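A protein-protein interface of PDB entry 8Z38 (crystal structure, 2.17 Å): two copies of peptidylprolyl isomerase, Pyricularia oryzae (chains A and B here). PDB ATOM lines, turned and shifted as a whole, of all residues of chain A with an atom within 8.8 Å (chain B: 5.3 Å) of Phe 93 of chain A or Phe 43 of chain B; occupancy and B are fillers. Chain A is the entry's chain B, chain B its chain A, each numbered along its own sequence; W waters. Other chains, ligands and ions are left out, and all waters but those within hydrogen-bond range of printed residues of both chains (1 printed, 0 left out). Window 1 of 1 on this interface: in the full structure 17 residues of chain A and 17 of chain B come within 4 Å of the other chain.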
ATOM      1  N   LEU A  30      33.817   6.182 -25.963  1.00  0.00           N
ATOM      2  CA  LEU A  30      34.468   5.887 -24.696  1.00  0.00           C
ATOM      3  C   LEU A  30      35.330   7.080 -24.321  1.00  0.00           C
ATOM      4  O   LEU A  30      36.042   7.624 -25.169  1.00  0.00           O
ATOM      5  CB  LEU A  30      35.311   4.621 -24.803  1.00  0.00           C
ATOM      6  CG  LEU A  30      34.529   3.400 -25.284  1.00  0.00           C
ATOM      7  CD1 LEU A  30      35.465   2.208 -25.445  1.00  0.00           C
ATOM      8  CD2 LEU A  30      33.423   3.080 -24.290  1.00  0.00           C
ATOM      9  N   PHE A  43      31.733   4.201 -30.321  1.00  0.00           N
ATOM     10  CA  PHE A  43      31.048   2.918 -30.376  1.00  0.00           C
ATOM     11  C   PHE A  43      29.678   2.984 -31.033  1.00  0.00           C
ATOM     12  O   PHE A  43      29.145   1.936 -31.400  1.00  0.00           O
ATOM     13  CB  PHE A  43      30.890   2.335 -28.974  1.00  0.00           C
ATOM     14  CG  PHE A  43      30.200   3.253 -28.026  1.00  0.00           C
ATOM     15  CD1 PHE A  43      28.825   3.236 -27.905  1.00  0.00           C
ATOM     16  CD2 PHE A  43      30.922   4.138 -27.258  1.00  0.00           C
ATOM     17  CE1 PHE A  43      28.187   4.082 -27.034  1.00  0.00           C
ATOM     18  CE2 PHE A  43      30.285   4.974 -26.383  1.00  0.00           C
ATOM     19  CZ  PHE A  43      28.912   4.947 -26.271  1.00  0.00           C
ATOM     20  N   TYR A  88      26.519   2.953 -18.293  1.00  0.00           N
ATOM     21  CA  TYR A  88      26.109   1.566 -18.159  1.00  0.00           C
ATOM     22  C   TYR A  88      26.666   0.909 -16.903  1.00  0.00           C
ATOM     23  O   TYR A  88      26.472  -0.293 -16.715  1.00  0.00           O
ATOM     24  CB  TYR A  88      26.501   0.803 -19.421  1.00  0.00           C
ATOM     25  CG  TYR A  88      25.727   1.317 -20.616  1.00  0.00           C
ATOM     26  CD1 TYR A  88      24.387   0.991 -20.775  1.00  0.00           C
ATOM     27  CD2 TYR A  88      26.321   2.143 -21.570  1.00  0.00           C
ATOM     28  CE1 TYR A  88      23.655   1.447 -21.858  1.00  0.00           C
ATOM     29  CE2 TYR A  88      25.586   2.618 -22.674  1.00  0.00           C
ATOM     30  CZ  TYR A  88      24.247   2.261 -22.801  1.00  0.00           C
ATOM     31  OH  TYR A  88      23.476   2.700 -23.865  1.00  0.00           O
ATOM     32  N   GLY A  89      27.326   1.672 -16.033  1.00  0.00           N
ATOM     33  CA  GLY A  89      27.746   1.144 -14.751  1.00  0.00           C
ATOM     34  C   GLY A  89      28.731   0.006 -14.893  1.00  0.00           C
ATOM     35  O   GLY A  89      29.660   0.044 -15.709  1.00  0.00           O
ATOM     36  N   ALA A  90      28.520  -1.030 -14.087  1.00  0.00           N
ATOM     37  CA  ALA A  90      29.406  -2.183 -14.034  1.00  0.00           C
ATOM     38  C   ALA A  90      29.138  -3.218 -15.127  1.00  0.00           C
ATOM     39  O   ALA A  90      29.813  -4.255 -15.152  1.00  0.00           O
ATOM     40  CB  ALA A  90      29.306  -2.847 -12.658  1.00  0.00           C
ATOM     41  N   ARG A  91      28.179  -2.998 -16.018  1.00  0.00           N
ATOM     42  CA  ARG A  91      28.010  -3.926 -17.128  1.00  0.00           C
ATOM     43  C   ARG A  91      28.584  -3.305 -18.392  1.00  0.00           C
ATOM     44  O   ARG A  91      28.674  -2.083 -18.519  1.00  0.00           O
ATOM     45  CB  ARG A  91      26.547  -4.331 -17.357  1.00  0.00           C
ATOM     46  CG  ARG A  91      26.446  -5.693 -18.130  1.00  0.00           C
ATOM     47  CD  ARG A  91      25.044  -6.299 -18.263  1.00  0.00           C
ATOM     48  NE  ARG A  91      24.223  -5.564 -19.217  1.00  0.00           N
ATOM     49  CZ  ARG A  91      22.897  -5.560 -19.210  1.00  0.00           C
ATOM     50  NH1 ARG A  91      22.205  -6.272 -18.330  1.00  0.00           N
ATOM     51  NH2 ARG A  91      22.249  -4.810 -20.095  1.00  0.00           N
ATOM     52  N   GLY A  92      29.017  -4.167 -19.307  1.00  0.00           N
ATOM     53  CA  GLY A  92      29.511  -3.714 -20.580  1.00  0.00           C
ATOM     54  C   GLY A  92      28.845  -4.438 -21.731  1.00  0.00           C
ATOM     55  O   GLY A  92      28.284  -5.523 -21.580  1.00  0.00           O
ATOM     56  N   PHE A  93      28.898  -3.797 -22.895  1.00  0.00           N
ATOM     57  CA  PHE A  93      28.508  -4.440 -24.138  1.00  0.00           C
ATOM     58  C   PHE A  93      29.777  -4.931 -24.815  1.00  0.00           C
ATOM     59  O   PHE A  93      30.591  -4.099 -25.248  1.00  0.00           O
ATOM     60  CB  PHE A  93      27.760  -3.459 -25.042  1.00  0.00           C
ATOM     61  CG  PHE A  93      27.126  -4.101 -26.251  1.00  0.00           C
ATOM     62  CD1 PHE A  93      27.874  -4.353 -27.400  1.00  0.00           C
ATOM     63  CD2 PHE A  93      25.789  -4.474 -26.232  1.00  0.00           C
ATOM     64  CE1 PHE A  93      27.291  -4.958 -28.513  1.00  0.00           C
ATOM     65  CE2 PHE A  93      25.210  -5.070 -27.340  1.00  0.00           C
ATOM     66  CZ  PHE A  93      25.964  -5.314 -28.480  1.00  0.00           C
ATOM     67  N   PRO A  94      29.992  -6.243 -24.922  1.00  0.00           N
ATOM     68  CA  PRO A  94      31.287  -6.762 -25.393  1.00  0.00           C
ATOM     69  C   PRO A  94      31.690  -6.214 -26.754  1.00  0.00           C
ATOM     70  O   PRO A  94      30.869  -6.094 -27.667  1.00  0.00           O
ATOM     71  CB  PRO A  94      31.064  -8.283 -25.448  1.00  0.00           C
ATOM     72  CG  PRO A  94      29.600  -8.504 -25.197  1.00  0.00           C
ATOM     73  CD  PRO A  94      29.093  -7.313 -24.462  1.00  0.00           C
ATOM     74  N   GLY A  95      32.981  -5.889 -26.880  1.00  0.00           N
ATOM     75  CA  GLY A  95      33.535  -5.290 -28.082  1.00  0.00           C
ATOM     76  C   GLY A  95      33.255  -3.812 -28.269  1.00  0.00           C
ATOM     77  O   GLY A  95      33.927  -3.169 -29.088  1.00  0.00           O
ATOM     78  N   ALA A  96      32.295  -3.247 -27.537  1.00  0.00           N
ATOM     79  CA  ALA A  96      31.934  -1.840 -27.661  1.00  0.00           C
ATOM     80  C   ALA A  96      32.231  -1.035 -26.405  1.00  0.00           C
ATOM     81  O   ALA A  96      32.933  -0.011 -26.475  1.00  0.00           O
ATOM     82  CB  ALA A  96      30.447  -1.713 -28.020  1.00  0.00           C
ATOM     83  N   ILE A  97      31.714  -1.463 -25.254  1.00  0.00           N
ATOM     84  CA  ILE A  97      31.807  -0.684 -24.019  1.00  0.00           C
ATOM     85  C   ILE A  97      32.262  -1.566 -22.862  1.00  0.00           C
ATOM     86  O   ILE A  97      31.446  -2.303 -22.300  1.00  0.00           O
ATOM     87  CB  ILE A  97      30.464  -0.021 -23.681  1.00  0.00           C
ATOM     88  CG1 ILE A  97      30.058   0.976 -24.763  1.00  0.00           C
ATOM     89  CG2 ILE A  97      30.533   0.683 -22.332  1.00  0.00           C
ATOM     90  CD1 ILE A  97      28.669   1.535 -24.562  1.00  0.00           C
ATOM     91  N   PRO A  98      33.521  -1.492 -22.437  1.00  0.00           N
ATOM     92  CA  PRO A  98      33.963  -2.263 -21.266  1.00  0.00           C
ATOM     93  C   PRO A  98      33.161  -1.896 -20.029  1.00  0.00           C
ATOM     94  O   PRO A  98      32.573  -0.806 -19.960  1.00  0.00           O
ATOM     95  CB  PRO A  98      35.436  -1.852 -21.106  1.00  0.00           C
ATOM     96  CG  PRO A  98      35.833  -1.285 -22.419  1.00  0.00           C
ATOM     97  CD  PRO A  98      34.601  -0.656 -22.988  1.00  0.00           C
ATOM     98  N   PRO A  99      33.098  -2.788 -19.034  1.00  0.00           N
ATOM     99  CA  PRO A  99      32.479  -2.425 -17.756  1.00  0.00           C
ATOM    100  C   PRO A  99      33.140  -1.200 -17.141  1.00  0.00           C
ATOM    101  O   PRO A  99      34.343  -0.977 -17.295  1.00  0.00           O
ATOM    102  CB  PRO A  99      32.699  -3.674 -16.892  1.00  0.00           C
ATOM    103  CG  PRO A  99      32.742  -4.807 -17.892  1.00  0.00           C
ATOM    104  CD  PRO A  99      33.461  -4.217 -19.086  1.00  0.00           C
ATOM    105  N   ASN A 100      32.327  -0.400 -16.446  1.00  0.00           N
ATOM    106  CA  ASN A 100      32.792   0.794 -15.731  1.00  0.00           C
ATOM    107  C   ASN A 100      33.473   1.794 -16.664  1.00  0.00           C
ATOM    108  O   ASN A 100      34.496   2.388 -16.322  1.00  0.00           O
ATOM    109  CB  ASN A 100      33.724   0.416 -14.578  1.00  0.00           C
ATOM    110  CG  ASN A 100      33.050  -0.481 -13.560  1.00  0.00           C
ATOM    111  OD1 ASN A 100      32.069  -0.089 -12.927  1.00  0.00           O
ATOM    112  ND2 ASN A 100      33.578  -1.695 -13.393  1.00  0.00           N
ATOM    113  N   SER A 101      32.905   1.988 -17.850  1.00  0.00           N
ATOM    114  CA  SER A 101      33.449   2.933 -18.820  1.00  0.00           C
ATOM    115  C   SER A 101      32.810   4.304 -18.633  1.00  0.00           C
ATOM    116  O   SER A 101      31.583   4.432 -18.688  1.00  0.00           O
ATOM    117  CB  SER A 101      33.203   2.445 -20.248  1.00  0.00           C
ATOM    118  OG  SER A 101      33.920   1.260 -20.528  1.00  0.00           O
ATOM    119  N   GLY B  28      26.457 -13.292 -31.941  1.00  0.00           N
ATOM    120  CA  GLY B  28      25.151 -12.951 -31.396  1.00  0.00           C
ATOM    121  C   GLY B  28      24.147 -12.669 -32.505  1.00  0.00           C
ATOM    122  O   GLY B  28      24.469 -12.012 -33.491  1.00  0.00           O
ATOM    123  N   PHE B  29      22.922 -13.156 -32.322  1.00  0.00           N
ATOM    124  CA  PHE B  29      21.846 -12.949 -33.284  1.00  0.00           C
ATOM    125  C   PHE B  29      20.588 -12.510 -32.556  1.00  0.00           C
ATOM    126  O   PHE B  29      20.283 -12.988 -31.457  1.00  0.00           O
ATOM    127  CB  PHE B  29      21.493 -14.217 -34.085  1.00  0.00           C
ATOM    128  CG  PHE B  29      22.650 -14.842 -34.787  1.00  0.00           C
ATOM    129  CD1 PHE B  29      23.383 -15.842 -34.180  1.00  0.00           C
ATOM    130  CD2 PHE B  29      22.992 -14.450 -36.068  1.00  0.00           C
ATOM    131  CE1 PHE B  29      24.456 -16.427 -34.832  1.00  0.00           C
ATOM    132  CE2 PHE B  29      24.060 -15.036 -36.724  1.00  0.00           C
ATOM    133  CZ  PHE B  29      24.793 -16.019 -36.104  1.00  0.00           C
ATOM    134  N   LEU B  30      19.840 -11.616 -33.193  1.00  0.00           N
ATOM    135  CA  LEU B  30      18.461 -11.411 -32.783  1.00  0.00           C
ATOM    136  C   LEU B  30      17.659 -12.667 -33.120  1.00  0.00           C
ATOM    137  O   LEU B  30      17.842 -13.276 -34.182  1.00  0.00           O
ATOM    138  CB  LEU B  30      17.867 -10.184 -33.475  1.00  0.00           C
ATOM    139  CG  LEU B  30      18.598  -8.852 -33.267  1.00  0.00           C
ATOM    140  CD1 LEU B  30      17.861  -7.724 -33.983  1.00  0.00           C
ATOM    141  CD2 LEU B  30      18.758  -8.538 -31.785  1.00  0.00           C
ATOM    142  N   ALA B  41      18.996 -11.318 -37.537  1.00  0.00           N
ATOM    143  CA  ALA B  41      20.160 -10.489 -37.821  1.00  0.00           C
ATOM    144  C   ALA B  41      21.273 -10.713 -36.800  1.00  0.00           C
ATOM    145  O   ALA B  41      21.043 -10.688 -35.585  1.00  0.00           O
ATOM    146  CB  ALA B  41      19.755  -9.012 -37.839  1.00  0.00           C
ATOM    147  N   GLN B  42      22.488 -10.913 -37.311  1.00  0.00           N
ATOM    148  CA  GLN B  42      23.693 -10.932 -36.489  1.00  0.00           C
ATOM    149  C   GLN B  42      24.030  -9.518 -36.032  1.00  0.00           C
ATOM    150  O   GLN B  42      24.199  -8.619 -36.862  1.00  0.00           O
ATOM    151  CB  GLN B  42      24.848 -11.521 -37.294  1.00  0.00           C
ATOM    152  CG  GLN B  42      26.229 -11.312 -36.686  1.00  0.00           C
ATOM    153  CD  GLN B  42      27.312 -12.053 -37.449  1.00  0.00           C
ATOM    154  OE1 GLN B  42      27.022 -12.892 -38.301  1.00  0.00           O
ATOM    155  NE2 GLN B  42      28.567 -11.753 -37.138  1.00  0.00           N
ATOM    156  N   PHE B  43      24.119  -9.304 -34.719  1.00  0.00           N
ATOM    157  CA  PHE B  43      24.467  -7.980 -34.222  1.00  0.00           C
ATOM    158  C   PHE B  43      25.894  -7.871 -33.710  1.00  0.00           C
ATOM    159  O   PHE B  43      26.457  -6.774 -33.745  1.00  0.00           O
ATOM    160  CB  PHE B  43      23.489  -7.525 -33.120  1.00  0.00           C
ATOM    161  CG  PHE B  43      23.502  -8.375 -31.879  1.00  0.00           C
ATOM    162  CD1 PHE B  43      24.340  -8.063 -30.815  1.00  0.00           C
ATOM    163  CD2 PHE B  43      22.652  -9.467 -31.758  1.00  0.00           C
ATOM    164  CE1 PHE B  43      24.345  -8.840 -29.669  1.00  0.00           C
ATOM    165  CE2 PHE B  43      22.645 -10.234 -30.606  1.00  0.00           C
ATOM    166  CZ  PHE B  43      23.494  -9.923 -29.565  1.00  0.00           C
ATOM    167  N   ASP B  44      26.502  -8.971 -33.272  1.00  0.00           N
ATOM    168  CA  ASP B  44      27.844  -8.904 -32.719  1.00  0.00           C
ATOM    169  C   ASP B  44      28.515 -10.258 -32.882  1.00  0.00           C
ATOM    170  O   ASP B  44      27.857 -11.277 -33.086  1.00  0.00           O
ATOM    171  CB  ASP B  44      27.826  -8.488 -31.245  1.00  0.00           C
ATOM    172  CG  ASP B  44      29.201  -8.080 -30.743  1.00  0.00           C
ATOM    173  OD1 ASP B  44      30.016  -7.631 -31.576  1.00  0.00           O
ATOM    174  OD2 ASP B  44      29.473  -8.225 -29.529  1.00  0.00           O
ATOM    175  N   SER B  45      29.839 -10.253 -32.775  1.00  0.00           N
ATOM    176  CA  SER B  45      30.626 -11.456 -32.978  1.00  0.00           C
ATOM    177  C   SER B  45      32.068 -11.179 -32.594  1.00  0.00           C
ATOM    178  O   SER B  45      32.613 -10.126 -32.930  1.00  0.00           O
ATOM    179  CB  SER B  45      30.563 -11.919 -34.433  1.00  0.00           C
ATOM    180  OG  SER B  45      31.304 -13.110 -34.599  1.00  0.00           O
ATOM    181  N   TYR B  88      19.118  -7.748 -22.929  1.00  0.00           N
ATOM    182  CA  TYR B  88      19.121  -6.310 -22.699  1.00  0.00           C
ATOM    183  C   TYR B  88      17.733  -5.782 -22.379  1.00  0.00           C
ATOM    184  O   TYR B  88      17.538  -4.571 -22.333  1.00  0.00           O
ATOM    185  CB  TYR B  88      19.732  -5.593 -23.901  1.00  0.00           C
ATOM    186  CG  TYR B  88      21.171  -6.012 -24.094  1.00  0.00           C
ATOM    187  CD1 TYR B  88      22.184  -5.476 -23.296  1.00  0.00           C
ATOM    188  CD2 TYR B  88      21.511  -6.989 -25.018  1.00  0.00           C
ATOM    189  CE1 TYR B  88      23.505  -5.873 -23.452  1.00  0.00           C
ATOM    190  CE2 TYR B  88      22.823  -7.404 -25.172  1.00  0.00           C
ATOM    191  CZ  TYR B  88      23.817  -6.840 -24.392  1.00  0.00           C
ATOM    192  OH  TYR B  88      25.125  -7.248 -24.554  1.00  0.00           O
ATOM    193  N   PHE B  93      19.850  -2.077 -26.378  1.00  0.00           N
ATOM    194  CA  PHE B  93      21.112  -1.348 -26.389  1.00  0.00           C
ATOM    195  C   PHE B  93      21.100  -0.421 -27.594  1.00  0.00           C
ATOM    196  O   PHE B  93      21.048  -0.909 -28.743  1.00  0.00           O
ATOM    197  CB  PHE B  93      22.305  -2.294 -26.445  1.00  0.00           C
ATOM    198  CG  PHE B  93      23.624  -1.609 -26.222  1.00  0.00           C
ATOM    199  CD1 PHE B  93      24.062  -1.337 -24.938  1.00  0.00           C
ATOM    200  CD2 PHE B  93      24.425  -1.246 -27.294  1.00  0.00           C
ATOM    201  CE1 PHE B  93      25.271  -0.711 -24.720  1.00  0.00           C
ATOM    202  CE2 PHE B  93      25.636  -0.620 -27.085  1.00  0.00           C
ATOM    203  CZ  PHE B  93      26.061  -0.355 -25.793  1.00  0.00           C
ATOM    204  N   ALA B  96      22.310  -1.070 -31.449  1.00  0.00           N
ATOM    205  CA  ALA B  96      22.695  -2.463 -31.631  1.00  0.00           C
ATOM    206  C   ALA B  96      21.523  -3.425 -31.504  1.00  0.00           C
ATOM    207  O   ALA B  96      21.327  -4.287 -32.364  1.00  0.00           O
ATOM    208  CB  ALA B  96      23.774  -2.842 -30.614  1.00  0.00           C
ATOM    209  N   ILE B  97      20.750  -3.311 -30.425  1.00  0.00           N
ATOM    210  CA  ILE B  97      19.743  -4.304 -30.082  1.00  0.00           C
ATOM    211  C   ILE B  97      18.422  -3.619 -29.762  1.00  0.00           C
ATOM    212  O   ILE B  97      18.356  -2.793 -28.850  1.00  0.00           O
ATOM    213  CB  ILE B  97      20.189  -5.186 -28.905  1.00  0.00           C
ATOM    214  CG1 ILE B  97      21.218  -6.199 -29.409  1.00  0.00           C
ATOM    215  CG2 ILE B  97      18.991  -5.880 -28.270  1.00  0.00           C
ATOM    216  CD1 ILE B  97      22.260  -6.479 -28.405  1.00  0.00           C
ATOM    217  N   LEU B 103      17.445 -13.223 -27.826  1.00  0.00           N
ATOM    218  CA  LEU B 103      18.768 -13.295 -28.422  1.00  0.00           C
ATOM    219  C   LEU B 103      19.167 -14.753 -28.596  1.00  0.00           C
ATOM    220  O   LEU B 103      18.771 -15.617 -27.815  1.00  0.00           O
ATOM    221  CB  LEU B 103      19.810 -12.556 -27.564  1.00  0.00           C
ATOM    222  CG  LEU B 103      19.437 -11.098 -27.214  1.00  0.00           C
ATOM    223  CD1 LEU B 103      20.392 -10.488 -26.181  1.00  0.00           C
ATOM    224  CD2 LEU B 103      19.372 -10.235 -28.477  1.00  0.00           C
ATOM    225  N   ILE B 104      19.949 -15.007 -29.641  1.00  0.00           N
ATOM    226  CA  ILE B 104      20.528 -16.309 -29.920  1.00  0.00           C
ATOM    227  C   ILE B 104      22.025 -16.103 -30.045  1.00  0.00           C
ATOM    228  O   ILE B 104      22.466 -15.282 -30.851  1.00  0.00           O
ATOM    229  CB  ILE B 104      19.969 -16.929 -31.217  1.00  0.00           C
ATOM    230  CG1 ILE B 104      18.447 -17.091 -31.159  1.00  0.00           C
ATOM    231  CG2 ILE B 104      20.646 -18.254 -31.505  1.00  0.00           C
ATOM    232  CD1 ILE B 104      17.994 -18.143 -30.202  1.00  0.00           C
ATOM    233  N   PHE B 105      22.802 -16.855 -29.269  1.00  0.00           N
ATOM    234  CA  PHE B 105      24.257 -16.779 -29.273  1.00  0.00           C
ATOM    235  C   PHE B 105      24.826 -18.150 -29.586  1.00  0.00           C
ATOM    236  O   PHE B 105      24.440 -19.134 -28.950  1.00  0.00           O
ATOM    237  CB  PHE B 105      24.797 -16.321 -27.911  1.00  0.00           C
ATOM    238  CG  PHE B 105      24.605 -14.863 -27.627  1.00  0.00           C
ATOM    239  CD1 PHE B 105      23.451 -14.406 -27.001  1.00  0.00           C
ATOM    240  CD2 PHE B 105      25.591 -13.944 -27.977  1.00  0.00           C
ATOM    241  CE1 PHE B 105      23.273 -13.042 -26.732  1.00  0.00           C
ATOM    242  CE2 PHE B 105      25.426 -12.580 -27.720  1.00  0.00           C
ATOM    243  CZ  PHE B 105      24.264 -12.128 -27.093  1.00  0.00           C
HETATM  244  O   HOH W   1      26.436  -8.069 -22.041  1.00  0.00           O
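The side-chain carboxylate of Asp 44 of chain B lies close to the backbone carbonyl oxygen of Pro 94 of chain A (3.2 Å).
O of Asp 44 of chain B is in hydrogen-bond range of N of Gly 28 of chain B, 2.7 Å away.
The backbone NH (N) of Phe 43 of chain B lies within hydrogen-bond range of the backbone carbonyl oxygen (O) of Gly 28 of chain B.
Among the printed residues, merely in contact across the chains: Tyr 88 of chain A with Phe 93 of chain B, Arg 91 of chain A with Tyr 88 of chain B, Phe 93 of chain A with Phe 43 of chain B, Phe 93 of chain A with Tyr 88 of chain B, Phe 93 of chain A with Phe 93 of chain B, Phe 93 of chain A with Ala 96 of chain B, Phe 93 of chain A with Ile 97 of chain B, Pro 94 of chain A with Tyr 88 of chain B and Ile 97 of chain A with Phe 93 of chain B.
Printed residues of chain B within 4 Å of Tyr 88 of chain A: Phe 93.
Phe 93 of chain A touches just these residues of chain B: Phe 43, Tyr 88, Phe 93, Ala 96 and Ile 97.
Printed residues of chain B within 4 Å of Pro 94 of chain A: Asp 44 and Tyr 88.
Of the printed residues of chain B, Ile 97 of chain A touches Phe 93.
Asp 44 of chain B touches one residue of chain A.
Printed residues of chain A within 4 Å of Tyr 88 of chain B: Arg 91, Phe 93 and Pro 94.
Printed residues of chain A within 4 Å of Ile 97 of chain B: Phe 93 (3.4 Å).
The nearest residue of chain B that does not touch Phe 93 of chain A is Asp 44 of chain B (4.1 Å).
The nearest residue of chain A that does not touch Phe 43 of chain B is Pro 94 of chain A (6.9 Å).
The nearest printed residue of chain A that does not touch Ala 96 of chain B is Phe 43 of chain A (7.2 Å).
Printed residues of chain B that touch a printed residue of chain A: Phe 43, Asp 44, Tyr 88, Phe 93, Ala 96 and Ile 97.
Of the 16 printed residues of chain A, 5 touch a printed residue of chain B.
Along chain A the printed residues that touch a printed residue of chain B span positions 88 to 97.
Tyr 88 of chain A touches Phe 93 of chain B, and with the chains exchanged Phe 93 of chain A touches Tyr 88 of chain B.
Phe 93 of chain A touches Phe 43 of chain B, but with the chains exchanged Phe 43 of chain A does not touch Phe 93 of chain B (5.0 Å).
Phe 93 of chain A touches Ala 96 of chain B, but with the chains exchanged Ala 96 of chain A does not touch Phe 93 of chain B (5.0 Å).
Phe 93 of chain A touches Ile 97 of chain B, and with the chains exchanged Ile 97 of chain A touches Phe 93 of chain B.
Positions printed for both chains: 30, 43, 88, 93, 96 and 97.
Water W1 lies within hydrogen-bond range of the side-chain hydroxyl (OH) of Tyr 88 of chain B (3.0 Å) and the backbone carbonyl oxygen (O) of Gly 92 of chain A (3.2 Å).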
